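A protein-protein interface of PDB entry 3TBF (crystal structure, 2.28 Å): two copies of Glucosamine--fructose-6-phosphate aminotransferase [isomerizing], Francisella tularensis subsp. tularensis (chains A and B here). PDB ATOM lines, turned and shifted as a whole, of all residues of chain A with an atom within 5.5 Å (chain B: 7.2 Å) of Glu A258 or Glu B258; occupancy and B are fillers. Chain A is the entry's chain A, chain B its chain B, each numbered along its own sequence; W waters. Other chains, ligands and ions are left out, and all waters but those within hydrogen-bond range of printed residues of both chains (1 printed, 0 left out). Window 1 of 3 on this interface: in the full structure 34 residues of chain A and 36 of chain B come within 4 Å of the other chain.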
ATOM      1  N   THR A 230      11.261  17.700 -16.401  1.00  0.00           N
ATOM      2  CA  THR A 230      11.097  19.103 -16.570  1.00  0.00           C
ATOM      3  C   THR A 230      10.934  19.766 -15.205  1.00  0.00           C
ATOM      4  O   THR A 230      10.281  19.244 -14.291  1.00  0.00           O
ATOM      5  CB  THR A 230       9.821  19.431 -17.381  1.00  0.00           C
ATOM      6  OG1 THR A 230       9.908  18.856 -18.706  1.00  0.00           O
ATOM      7  CG2 THR A 230       9.622  20.955 -17.452  1.00  0.00           C
ATOM      8  N   ILE A 231      11.477  20.966 -15.114  1.00  0.00           N
ATOM      9  CA  ILE A 231      11.262  21.806 -13.985  1.00  0.00           C
ATOM     10  C   ILE A 231      10.397  23.025 -14.283  1.00  0.00           C
ATOM     11  O   ILE A 231      10.612  23.731 -15.272  1.00  0.00           O
ATOM     12  CB  ILE A 231      12.582  22.286 -13.499  1.00  0.00           C
ATOM     13  CG1 ILE A 231      13.429  21.053 -13.146  1.00  0.00           C
ATOM     14  CG2 ILE A 231      12.390  23.277 -12.337  1.00  0.00           C
ATOM     15  CD1 ILE A 231      14.335  21.270 -12.017  1.00  0.00           C
ATOM     16  N   PHE A 232       9.415  23.257 -13.410  1.00  0.00           N
ATOM     17  CA  PHE A 232       8.527  24.398 -13.498  1.00  0.00           C
ATOM     18  C   PHE A 232       8.893  25.355 -12.361  1.00  0.00           C
ATOM     19  O   PHE A 232       9.207  24.914 -11.247  1.00  0.00           O
ATOM     20  CB  PHE A 232       7.076  23.990 -13.373  1.00  0.00           C
ATOM     21  CG  PHE A 232       6.498  23.407 -14.616  1.00  0.00           C
ATOM     22  CD1 PHE A 232       6.881  22.163 -15.064  1.00  0.00           C
ATOM     23  CD2 PHE A 232       5.525  24.074 -15.319  1.00  0.00           C
ATOM     24  CE1 PHE A 232       6.326  21.597 -16.214  1.00  0.00           C
ATOM     25  CE2 PHE A 232       4.987  23.524 -16.501  1.00  0.00           C
ATOM     26  CZ  PHE A 232       5.401  22.302 -16.956  1.00  0.00           C
ATOM     27  N   ALA A 246       2.998  21.663 -13.777  1.00  0.00           N
ATOM     28  CA  ALA A 246       3.799  20.430 -13.660  1.00  0.00           C
ATOM     29  C   ALA A 246       2.899  19.259 -13.518  1.00  0.00           C
ATOM     30  O   ALA A 246       3.179  18.218 -14.059  1.00  0.00           O
ATOM     31  CB  ALA A 246       4.797  20.491 -12.474  1.00  0.00           C
ATOM     32  N   LYS A 250       2.950  16.018 -16.114  1.00  0.00           N
ATOM     33  CA  LYS A 250       3.211  14.722 -15.534  1.00  0.00           C
ATOM     34  C   LYS A 250       2.038  13.776 -15.808  1.00  0.00           C
ATOM     35  O   LYS A 250       2.220  12.646 -16.283  1.00  0.00           O
ATOM     36  CB  LYS A 250       3.413  14.959 -14.025  1.00  0.00           C
ATOM     37  CG  LYS A 250       3.724  13.802 -13.158  1.00  0.00           C
ATOM     38  CD  LYS A 250       4.227  14.242 -11.769  1.00  0.00           C
ATOM     39  CE  LYS A 250       3.494  15.476 -11.189  1.00  0.00           C
ATOM     40  NZ  LYS A 250       3.850  15.755  -9.760  1.00  0.00           N
ATOM     41  N   HIS A 256       8.584  13.382 -15.875  1.00  0.00           N
ATOM     42  CA  HIS A 256       8.760  13.700 -14.470  1.00  0.00           C
ATOM     43  C   HIS A 256       8.884  15.207 -14.299  1.00  0.00           C
ATOM     44  O   HIS A 256       9.986  15.753 -14.204  1.00  0.00           O
ATOM     45  CB  HIS A 256       9.974  12.978 -13.860  1.00  0.00           C
ATOM     46  CG  HIS A 256      10.014  13.021 -12.359  1.00  0.00           C
ATOM     47  ND1 HIS A 256      11.022  12.439 -11.627  1.00  0.00           N
ATOM     48  CD2 HIS A 256       9.167  13.572 -11.456  1.00  0.00           C
ATOM     49  CE1 HIS A 256      10.788  12.627 -10.340  1.00  0.00           C
ATOM     50  NE2 HIS A 256       9.686  13.334 -10.210  1.00  0.00           N
ATOM     51  N   ALA A 257       7.746  15.873 -14.197  1.00  0.00           N
ATOM     52  CA  ALA A 257       7.715  17.305 -14.118  1.00  0.00           C
ATOM     53  C   ALA A 257       7.580  17.624 -12.676  1.00  0.00           C
ATOM     54  O   ALA A 257       6.792  16.999 -12.012  1.00  0.00           O
ATOM     55  CB  ALA A 257       6.516  17.840 -14.871  1.00  0.00           C
ATOM     56  N   GLU A 258       8.344  18.599 -12.195  1.00  0.00           N
ATOM     57  CA  GLU A 258       8.242  19.068 -10.848  1.00  0.00           C
ATOM     58  C   GLU A 258       8.381  20.582 -10.752  1.00  0.00           C
ATOM     59  O   GLU A 258       9.232  21.209 -11.450  1.00  0.00           O
ATOM     60  CB  GLU A 258       9.361  18.429 -10.027  1.00  0.00           C
ATOM     61  CG  GLU A 258       9.133  18.634  -8.531  1.00  0.00           C
ATOM     62  CD  GLU A 258      10.234  18.048  -7.679  1.00  0.00           C
ATOM     63  OE1 GLU A 258      11.234  17.610  -8.303  1.00  0.00           O
ATOM     64  OE2 GLU A 258      10.111  18.065  -6.420  1.00  0.00           O
ATOM     65  N   ALA A 259       7.589  21.159  -9.843  1.00  0.00           N
ATOM     66  CA  ALA A 259       7.569  22.603  -9.608  1.00  0.00           C
ATOM     67  C   ALA A 259       8.304  22.993  -8.349  1.00  0.00           C
ATOM     68  O   ALA A 259       8.174  22.333  -7.320  1.00  0.00           O
ATOM     69  CB  ALA A 259       6.156  23.126  -9.542  1.00  0.00           C
ATOM     70  N   TYR A 260       9.026  24.100  -8.439  1.00  0.00           N
ATOM     71  CA  TYR A 260       9.742  24.680  -7.291  1.00  0.00           C
ATOM     72  C   TYR A 260       9.418  26.163  -7.203  1.00  0.00           C
ATOM     73  O   TYR A 260       9.269  26.810  -8.243  1.00  0.00           O
ATOM     74  CB  TYR A 260      11.227  24.503  -7.475  1.00  0.00           C
ATOM     75  CG  TYR A 260      11.709  23.053  -7.389  1.00  0.00           C
ATOM     76  CD1 TYR A 260      12.080  22.483  -6.161  1.00  0.00           C
ATOM     77  CD2 TYR A 260      11.864  22.283  -8.543  1.00  0.00           C
ATOM     78  CE1 TYR A 260      12.542  21.185  -6.095  1.00  0.00           C
ATOM     79  CE2 TYR A 260      12.298  20.997  -8.493  1.00  0.00           C
ATOM     80  CZ  TYR A 260      12.659  20.439  -7.273  1.00  0.00           C
ATOM     81  OH  TYR A 260      13.142  19.128  -7.257  1.00  0.00           O
ATOM     82  N   LEU A 272      19.863  19.327 -10.062  1.00  0.00           N
ATOM     83  CA  LEU A 272      19.231  18.562 -11.149  1.00  0.00           C
ATOM     84  C   LEU A 272      19.396  19.165 -12.557  1.00  0.00           C
ATOM     85  O   LEU A 272      19.289  18.454 -13.578  1.00  0.00           O
ATOM     86  CB  LEU A 272      17.735  18.398 -10.857  1.00  0.00           C
ATOM     87  CG  LEU A 272      17.340  17.611  -9.608  1.00  0.00           C
ATOM     88  CD1 LEU A 272      15.817  17.428  -9.600  1.00  0.00           C
ATOM     89  CD2 LEU A 272      18.065  16.258  -9.567  1.00  0.00           C
ATOM     90  N   HIS B 229      15.712   8.682 -11.551  1.00  0.00           N
ATOM     91  CA  HIS B 229      14.530   9.058 -10.803  1.00  0.00           C
ATOM     92  C   HIS B 229      14.445   8.235  -9.521  1.00  0.00           C
ATOM     93  O   HIS B 229      14.917   7.111  -9.485  1.00  0.00           O
ATOM     94  CB  HIS B 229      13.290   8.728 -11.618  1.00  0.00           C
ATOM     95  CG  HIS B 229      13.269   9.327 -12.989  1.00  0.00           C
ATOM     96  ND1 HIS B 229      12.754  10.575 -13.241  1.00  0.00           N
ATOM     97  CD2 HIS B 229      13.653   8.829 -14.189  1.00  0.00           C
ATOM     98  CE1 HIS B 229      12.871  10.842 -14.535  1.00  0.00           C
ATOM     99  NE2 HIS B 229      13.394   9.792 -15.136  1.00  0.00           N
ATOM    100  N   THR B 230      13.830   8.791  -8.481  1.00  0.00           N
ATOM    101  CA  THR B 230      13.321   8.002  -7.379  1.00  0.00           C
ATOM    102  C   THR B 230      12.134   8.688  -6.734  1.00  0.00           C
ATOM    103  O   THR B 230      12.107   9.918  -6.662  1.00  0.00           O
ATOM    104  CB  THR B 230      14.372   7.779  -6.289  1.00  0.00           C
ATOM    105  OG1 THR B 230      15.556   7.199  -6.859  1.00  0.00           O
ATOM    106  CG2 THR B 230      13.812   6.890  -5.232  1.00  0.00           C
ATOM    107  N   ILE B 231      11.146   7.905  -6.287  1.00  0.00           N
ATOM    108  CA  ILE B 231      10.021   8.442  -5.533  1.00  0.00           C
ATOM    109  C   ILE B 231      10.090   8.079  -4.075  1.00  0.00           C
ATOM    110  O   ILE B 231      10.330   6.913  -3.735  1.00  0.00           O
ATOM    111  CB  ILE B 231       8.685   7.878  -6.042  1.00  0.00           C
ATOM    112  CG1 ILE B 231       8.372   8.387  -7.447  1.00  0.00           C
ATOM    113  CG2 ILE B 231       7.525   8.259  -5.093  1.00  0.00           C
ATOM    114  CD1 ILE B 231       7.171   7.666  -7.996  1.00  0.00           C
ATOM    115  N   PHE B 232       9.897   9.068  -3.206  1.00  0.00           N
ATOM    116  CA  PHE B 232       9.848   8.825  -1.766  1.00  0.00           C
ATOM    117  C   PHE B 232       8.394   8.937  -1.270  1.00  0.00           C
ATOM    118  O   PHE B 232       7.642   9.791  -1.728  1.00  0.00           O
ATOM    119  CB  PHE B 232      10.713   9.832  -1.033  1.00  0.00           C
ATOM    120  CG  PHE B 232      12.182   9.527  -1.068  1.00  0.00           C
ATOM    121  CD1 PHE B 232      12.918   9.719  -2.218  1.00  0.00           C
ATOM    122  CD2 PHE B 232      12.827   9.071   0.048  1.00  0.00           C
ATOM    123  CE1 PHE B 232      14.251   9.436  -2.256  1.00  0.00           C
ATOM    124  CE2 PHE B 232      14.168   8.790   0.019  1.00  0.00           C
ATOM    125  CZ  PHE B 232      14.885   9.002  -1.134  1.00  0.00           C
ATOM    126  N   LEU B 233       7.997   8.062  -0.356  1.00  0.00           N
ATOM    127  CA  LEU B 233       6.613   8.058   0.142  1.00  0.00           C
ATOM    128  C   LEU B 233       6.579   8.064   1.646  1.00  0.00           C
ATOM    129  O   LEU B 233       7.353   7.385   2.300  1.00  0.00           O
ATOM    130  CB  LEU B 233       5.819   6.827  -0.346  1.00  0.00           C
ATOM    131  CG  LEU B 233       5.644   6.648  -1.864  1.00  0.00           C
ATOM    132  CD1 LEU B 233       4.861   5.398  -2.110  1.00  0.00           C
ATOM    133  CD2 LEU B 233       4.952   7.814  -2.554  1.00  0.00           C
ATOM    134  N   ALA B 242       9.890  11.977   4.394  1.00  0.00           N
ATOM    135  CA  ALA B 242      10.136  11.515   3.002  1.00  0.00           C
ATOM    136  C   ALA B 242      10.671  12.657   2.170  1.00  0.00           C
ATOM    137  O   ALA B 242      11.570  12.473   1.380  1.00  0.00           O
ATOM    138  CB  ALA B 242       8.930  10.921   2.365  1.00  0.00           C
ATOM    139  N   ILE B 243      10.179  13.851   2.405  1.00  0.00           N
ATOM    140  CA  ILE B 243      10.637  15.003   1.635  1.00  0.00           C
ATOM    141  C   ILE B 243      12.102  15.274   1.935  1.00  0.00           C
ATOM    142  O   ILE B 243      12.900  15.613   1.076  1.00  0.00           O
ATOM    143  CB  ILE B 243       9.823  16.249   1.971  1.00  0.00           C
ATOM    144  CG1 ILE B 243       8.387  16.193   1.410  1.00  0.00           C
ATOM    145  CG2 ILE B 243      10.439  17.514   1.388  1.00  0.00           C
ATOM    146  CD1 ILE B 243       7.517  17.351   1.982  1.00  0.00           C
ATOM    147  N   ALA B 246      14.262  12.718   0.113  1.00  0.00           N
ATOM    148  CA  ALA B 246      14.329  13.120  -1.285  1.00  0.00           C
ATOM    149  C   ALA B 246      15.326  14.275  -1.479  1.00  0.00           C
ATOM    150  O   ALA B 246      16.139  14.277  -2.415  1.00  0.00           O
ATOM    151  CB  ALA B 246      12.961  13.535  -1.761  1.00  0.00           C
ATOM    152  N   LEU B 247      15.293  15.235  -0.558  1.00  0.00           N
ATOM    153  CA  LEU B 247      16.152  16.417  -0.659  1.00  0.00           C
ATOM    154  C   LEU B 247      17.609  15.998  -0.588  1.00  0.00           C
ATOM    155  O   LEU B 247      18.384  16.471  -1.348  1.00  0.00           O
ATOM    156  CB  LEU B 247      15.859  17.377   0.489  1.00  0.00           C
ATOM    157  CG  LEU B 247      16.693  18.636   0.606  1.00  0.00           C
ATOM    158  CD1 LEU B 247      16.510  19.401  -0.653  1.00  0.00           C
ATOM    159  CD2 LEU B 247      16.321  19.505   1.809  1.00  0.00           C
ATOM    160  N   LEU B 249      18.944  12.955  -1.312  1.00  0.00           N
ATOM    161  CA  LEU B 249      19.338  12.156  -2.430  1.00  0.00           C
ATOM    162  C   LEU B 249      19.584  13.047  -3.662  1.00  0.00           C
ATOM    163  O   LEU B 249      20.568  12.914  -4.398  1.00  0.00           O
ATOM    164  CB  LEU B 249      18.231  11.158  -2.732  1.00  0.00           C
ATOM    165  CG  LEU B 249      18.611  10.098  -3.756  1.00  0.00           C
ATOM    166  CD1 LEU B 249      19.949   9.394  -3.259  1.00  0.00           C
ATOM    167  CD2 LEU B 249      17.457   9.106  -3.967  1.00  0.00           C
ATOM    168  N   LYS B 250      18.669  13.963  -3.890  1.00  0.00           N
ATOM    169  CA  LYS B 250      18.801  14.914  -4.973  1.00  0.00           C
ATOM    170  C   LYS B 250      20.068  15.796  -4.844  1.00  0.00           C
ATOM    171  O   LYS B 250      20.814  16.009  -5.803  1.00  0.00           O
ATOM    172  CB  LYS B 250      17.541  15.770  -4.913  1.00  0.00           C
ATOM    173  CG  LYS B 250      17.365  16.750  -5.914  1.00  0.00           C
ATOM    174  CD  LYS B 250      15.947  17.389  -5.832  1.00  0.00           C
ATOM    175  CE  LYS B 250      15.291  17.307  -4.436  1.00  0.00           C
ATOM    176  NZ  LYS B 250      14.240  18.319  -4.211  1.00  0.00           N
ATOM    177  N   ILE B 255      20.235  12.485  -8.400  1.00  0.00           N
ATOM    178  CA  ILE B 255      19.038  11.782  -8.869  1.00  0.00           C
ATOM    179  C   ILE B 255      17.801  12.671  -8.733  1.00  0.00           C
ATOM    180  O   ILE B 255      17.674  13.443  -7.766  1.00  0.00           O
ATOM    181  CB  ILE B 255      18.789  10.499  -8.065  1.00  0.00           C
ATOM    182  CG1 ILE B 255      19.756   9.413  -8.541  1.00  0.00           C
ATOM    183  CG2 ILE B 255      17.384   9.995  -8.246  1.00  0.00           C
ATOM    184  CD1 ILE B 255      20.022   8.295  -7.586  1.00  0.00           C
ATOM    185  N   HIS B 256      16.865  12.546  -9.668  1.00  0.00           N
ATOM    186  CA  HIS B 256      15.639  13.305  -9.565  1.00  0.00           C
ATOM    187  C   HIS B 256      14.694  12.598  -8.611  1.00  0.00           C
ATOM    188  O   HIS B 256      13.845  11.811  -9.010  1.00  0.00           O
ATOM    189  CB  HIS B 256      14.998  13.530 -10.931  1.00  0.00           C
ATOM    190  CG  HIS B 256      13.885  14.544 -10.912  1.00  0.00           C
ATOM    191  ND1 HIS B 256      13.234  14.952 -12.052  1.00  0.00           N
ATOM    192  CD2 HIS B 256      13.315  15.229  -9.889  1.00  0.00           C
ATOM    193  CE1 HIS B 256      12.302  15.827 -11.731  1.00  0.00           C
ATOM    194  NE2 HIS B 256      12.333  16.017 -10.426  1.00  0.00           N
ATOM    195  N   ALA B 257      14.894  12.877  -7.331  1.00  0.00           N
ATOM    196  CA  ALA B 257      14.153  12.265  -6.256  1.00  0.00           C
ATOM    197  C   ALA B 257      13.016  13.185  -5.882  1.00  0.00           C
ATOM    198  O   ALA B 257      13.204  14.390  -5.741  1.00  0.00           O
ATOM    199  CB  ALA B 257      15.053  12.090  -5.058  1.00  0.00           C
ATOM    200  N   GLU B 258      11.834  12.634  -5.697  1.00  0.00           N
ATOM    201  CA  GLU B 258      10.704  13.450  -5.296  1.00  0.00           C
ATOM    202  C   GLU B 258       9.882  12.731  -4.294  1.00  0.00           C
ATOM    203  O   GLU B 258       9.686  11.570  -4.469  1.00  0.00           O
ATOM    204  CB  GLU B 258       9.790  13.740  -6.491  1.00  0.00           C
ATOM    205  CG  GLU B 258       8.749  14.871  -6.176  1.00  0.00           C
ATOM    206  CD  GLU B 258       7.903  15.288  -7.393  1.00  0.00           C
ATOM    207  OE1 GLU B 258       7.990  14.594  -8.438  1.00  0.00           O
ATOM    208  OE2 GLU B 258       7.132  16.293  -7.276  1.00  0.00           O
ATOM    209  N   ALA B 259       9.381  13.438  -3.292  1.00  0.00           N
ATOM    210  CA  ALA B 259       8.506  12.862  -2.285  1.00  0.00           C
ATOM    211  C   ALA B 259       7.044  13.208  -2.541  1.00  0.00           C
ATOM    212  O   ALA B 259       6.741  14.326  -2.935  1.00  0.00           O
ATOM    213  CB  ALA B 259       8.875  13.360  -0.914  1.00  0.00           C
ATOM    214  N   TYR B 260       6.171  12.254  -2.246  1.00  0.00           N
ATOM    215  CA  TYR B 260       4.744  12.425  -2.321  1.00  0.00           C
ATOM    216  C   TYR B 260       4.085  11.895  -1.068  1.00  0.00           C
ATOM    217  O   TYR B 260       4.540  10.924  -0.504  1.00  0.00           O
ATOM    218  CB  TYR B 260       4.188  11.628  -3.496  1.00  0.00           C
ATOM    219  CG  TYR B 260       4.536  12.160  -4.846  1.00  0.00           C
ATOM    220  CD1 TYR B 260       3.779  13.177  -5.428  1.00  0.00           C
ATOM    221  CD2 TYR B 260       5.612  11.654  -5.560  1.00  0.00           C
ATOM    222  CE1 TYR B 260       4.109  13.702  -6.686  1.00  0.00           C
ATOM    223  CE2 TYR B 260       5.950  12.163  -6.801  1.00  0.00           C
ATOM    224  CZ  TYR B 260       5.195  13.186  -7.370  1.00  0.00           C
ATOM    225  OH  TYR B 260       5.497  13.706  -8.632  1.00  0.00           O
ATOM    226  N   PRO B 269       1.510  11.156  -9.874  1.00  0.00           N
ATOM    227  CA  PRO B 269       2.635  10.359  -9.351  1.00  0.00           C
ATOM    228  C   PRO B 269       2.591   8.850  -9.668  1.00  0.00           C
ATOM    229  O   PRO B 269       3.641   8.226  -9.785  1.00  0.00           O
ATOM    230  CB  PRO B 269       2.557  10.590  -7.839  1.00  0.00           C
ATOM    231  CG  PRO B 269       1.222  11.235  -7.603  1.00  0.00           C
ATOM    232  CD  PRO B 269       0.857  11.958  -8.828  1.00  0.00           C
ATOM    233  N   LEU B 272       4.041   7.894 -13.195  1.00  0.00           N
ATOM    234  CA  LEU B 272       5.491   7.945 -13.375  1.00  0.00           C
ATOM    235  C   LEU B 272       6.167   6.658 -12.993  1.00  0.00           C
ATOM    236  O   LEU B 272       7.330   6.453 -13.330  1.00  0.00           O
ATOM    237  CB  LEU B 272       6.085   9.041 -12.512  1.00  0.00           C
ATOM    238  CG  LEU B 272       5.697  10.453 -12.897  1.00  0.00           C
ATOM    239  CD1 LEU B 272       6.077  11.437 -11.805  1.00  0.00           C
ATOM    240  CD2 LEU B 272       6.352  10.768 -14.216  1.00  0.00           C
ATOM    241  N   VAL B 280      11.230   4.468  -2.410  1.00  0.00           N
ATOM    242  CA  VAL B 280      11.718   4.443  -1.064  1.00  0.00           C
ATOM    243  C   VAL B 280      10.570   4.874  -0.151  1.00  0.00           C
ATOM    244  O   VAL B 280       9.990   5.944  -0.308  1.00  0.00           O
ATOM    245  CB  VAL B 280      12.868   5.408  -0.885  1.00  0.00           C
ATOM    246  CG1 VAL B 280      13.410   5.295   0.547  1.00  0.00           C
ATOM    247  CG2 VAL B 280      13.966   5.169  -1.906  1.00  0.00           C
HETATM  248  O   HOH W   1      12.006  16.895  -4.961  1.00  0.00           O
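The backbone NH (N) of Thr A230 lies within hydrogen-bond range of the backbone carbonyl oxygen (O) of His A256, at 3.2 Å.
N of Phe A232 is in hydrogen-bond range of O of Glu A258, at 2.8 Å.
The backbone carbonyl oxygen of Phe A232 is in hydrogen-bond range of the backbone NH of Tyr A260 (2.9 Å).
The side-chain carboxylate of Glu A258 lies within hydrogen-bond range of the side-chain hydroxyl of Tyr A260 (2.7 Å).
N of Phe B232 lies within hydrogen-bond range of O of Glu B258 (2.8 Å).
OH of Tyr B260 lies within hydrogen-bond range of OE1 of Glu B258, at 2.7 Å.
The side-chain amino group (NZ) of Lys A250 is in hydrogen-bond range of the side-chain hydroxyl (OH) of Tyr B260 (2.9 Å).
A ring nitrogen (ND1) of His A256 sits at hydrogen-bond distance from a ring nitrogen (ND1) of His B229, 3.0 Å away.
A ring nitrogen (ND1) of His B256 is in hydrogen-bond range of a ring nitrogen (ND1) of His A256, at 3.4 Å.
OE1 of Glu B258 is in hydrogen-bond range of NE2 of His A256.
NE2 of His B256 sits at hydrogen-bond distance from OE1 of Glu A258.
OH of Tyr A260 lies within hydrogen-bond range of NZ of Lys B250.
Of the printed residues of chain B, Lys A250 touches Tyr B260 and Leu B272.
Of the printed residues of chain B, His A256 touches His B229 (3.0 Å), His B256 (3.4 Å), Glu B258 (2.8 Å) and Leu B272 (3.8 Å).
Of chain B, only His B256 and Glu B258 come within 4 Å of Glu A258.
Of the printed residues of chain B, Leu A272 touches Lys B250 (3.8 Å), Ile B255 (3.4 Å) and His B256 (3.3 Å).
Printed residues of chain A within 4 Å of His B229: His A256.
Glu B258 touches just these residues of chain A: His A256 and Glu A258.
The nearest printed residue of chain B that does not touch Leu A272 is Ala B257 (5.1 Å).
Of the 20 printed residues of chain B, 7 touch a printed residue of chain A.
Hydrophobic or aromatic side chains of chain B within 4 Å of the printed part of chain A: His B229, His B256, Tyr B260 and Leu B272.
Among the printed residues, 12 pairs touch across the chains.
Among the printed residues, merely in contact across the chains: Lys A250 with Leu B272 (3.4 Å), His A256 with Leu B272 (3.8 Å), Glu A258 with Glu B258 (3.3 Å), Leu A272 with Lys B250 (3.8 Å), Leu A272 with Ile B255 (3.4 Å) and Leu A272 with His B256 (3.3 Å).
His B256 touches its own counterpart, His A256.
His A256 touches Glu B258, and with the chains exchanged Glu A258 touches His B256.
His A256 touches Leu B272, and with the chains exchanged Leu A272 touches His B256.
Glu B258 touches its own counterpart, Glu A258.
Water W1 lies within hydrogen-bond range of the side-chain carboxylate (OE2) of Glu A258 (2.7 Å), the side-chain amino group (NZ) of Lys B250 (2.8 Å), the backbone carbonyl oxygen (O) of Ala B257 (2.9 Å) and the side-chain hydroxyl (OH) of Tyr A260 (3.4 Å).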
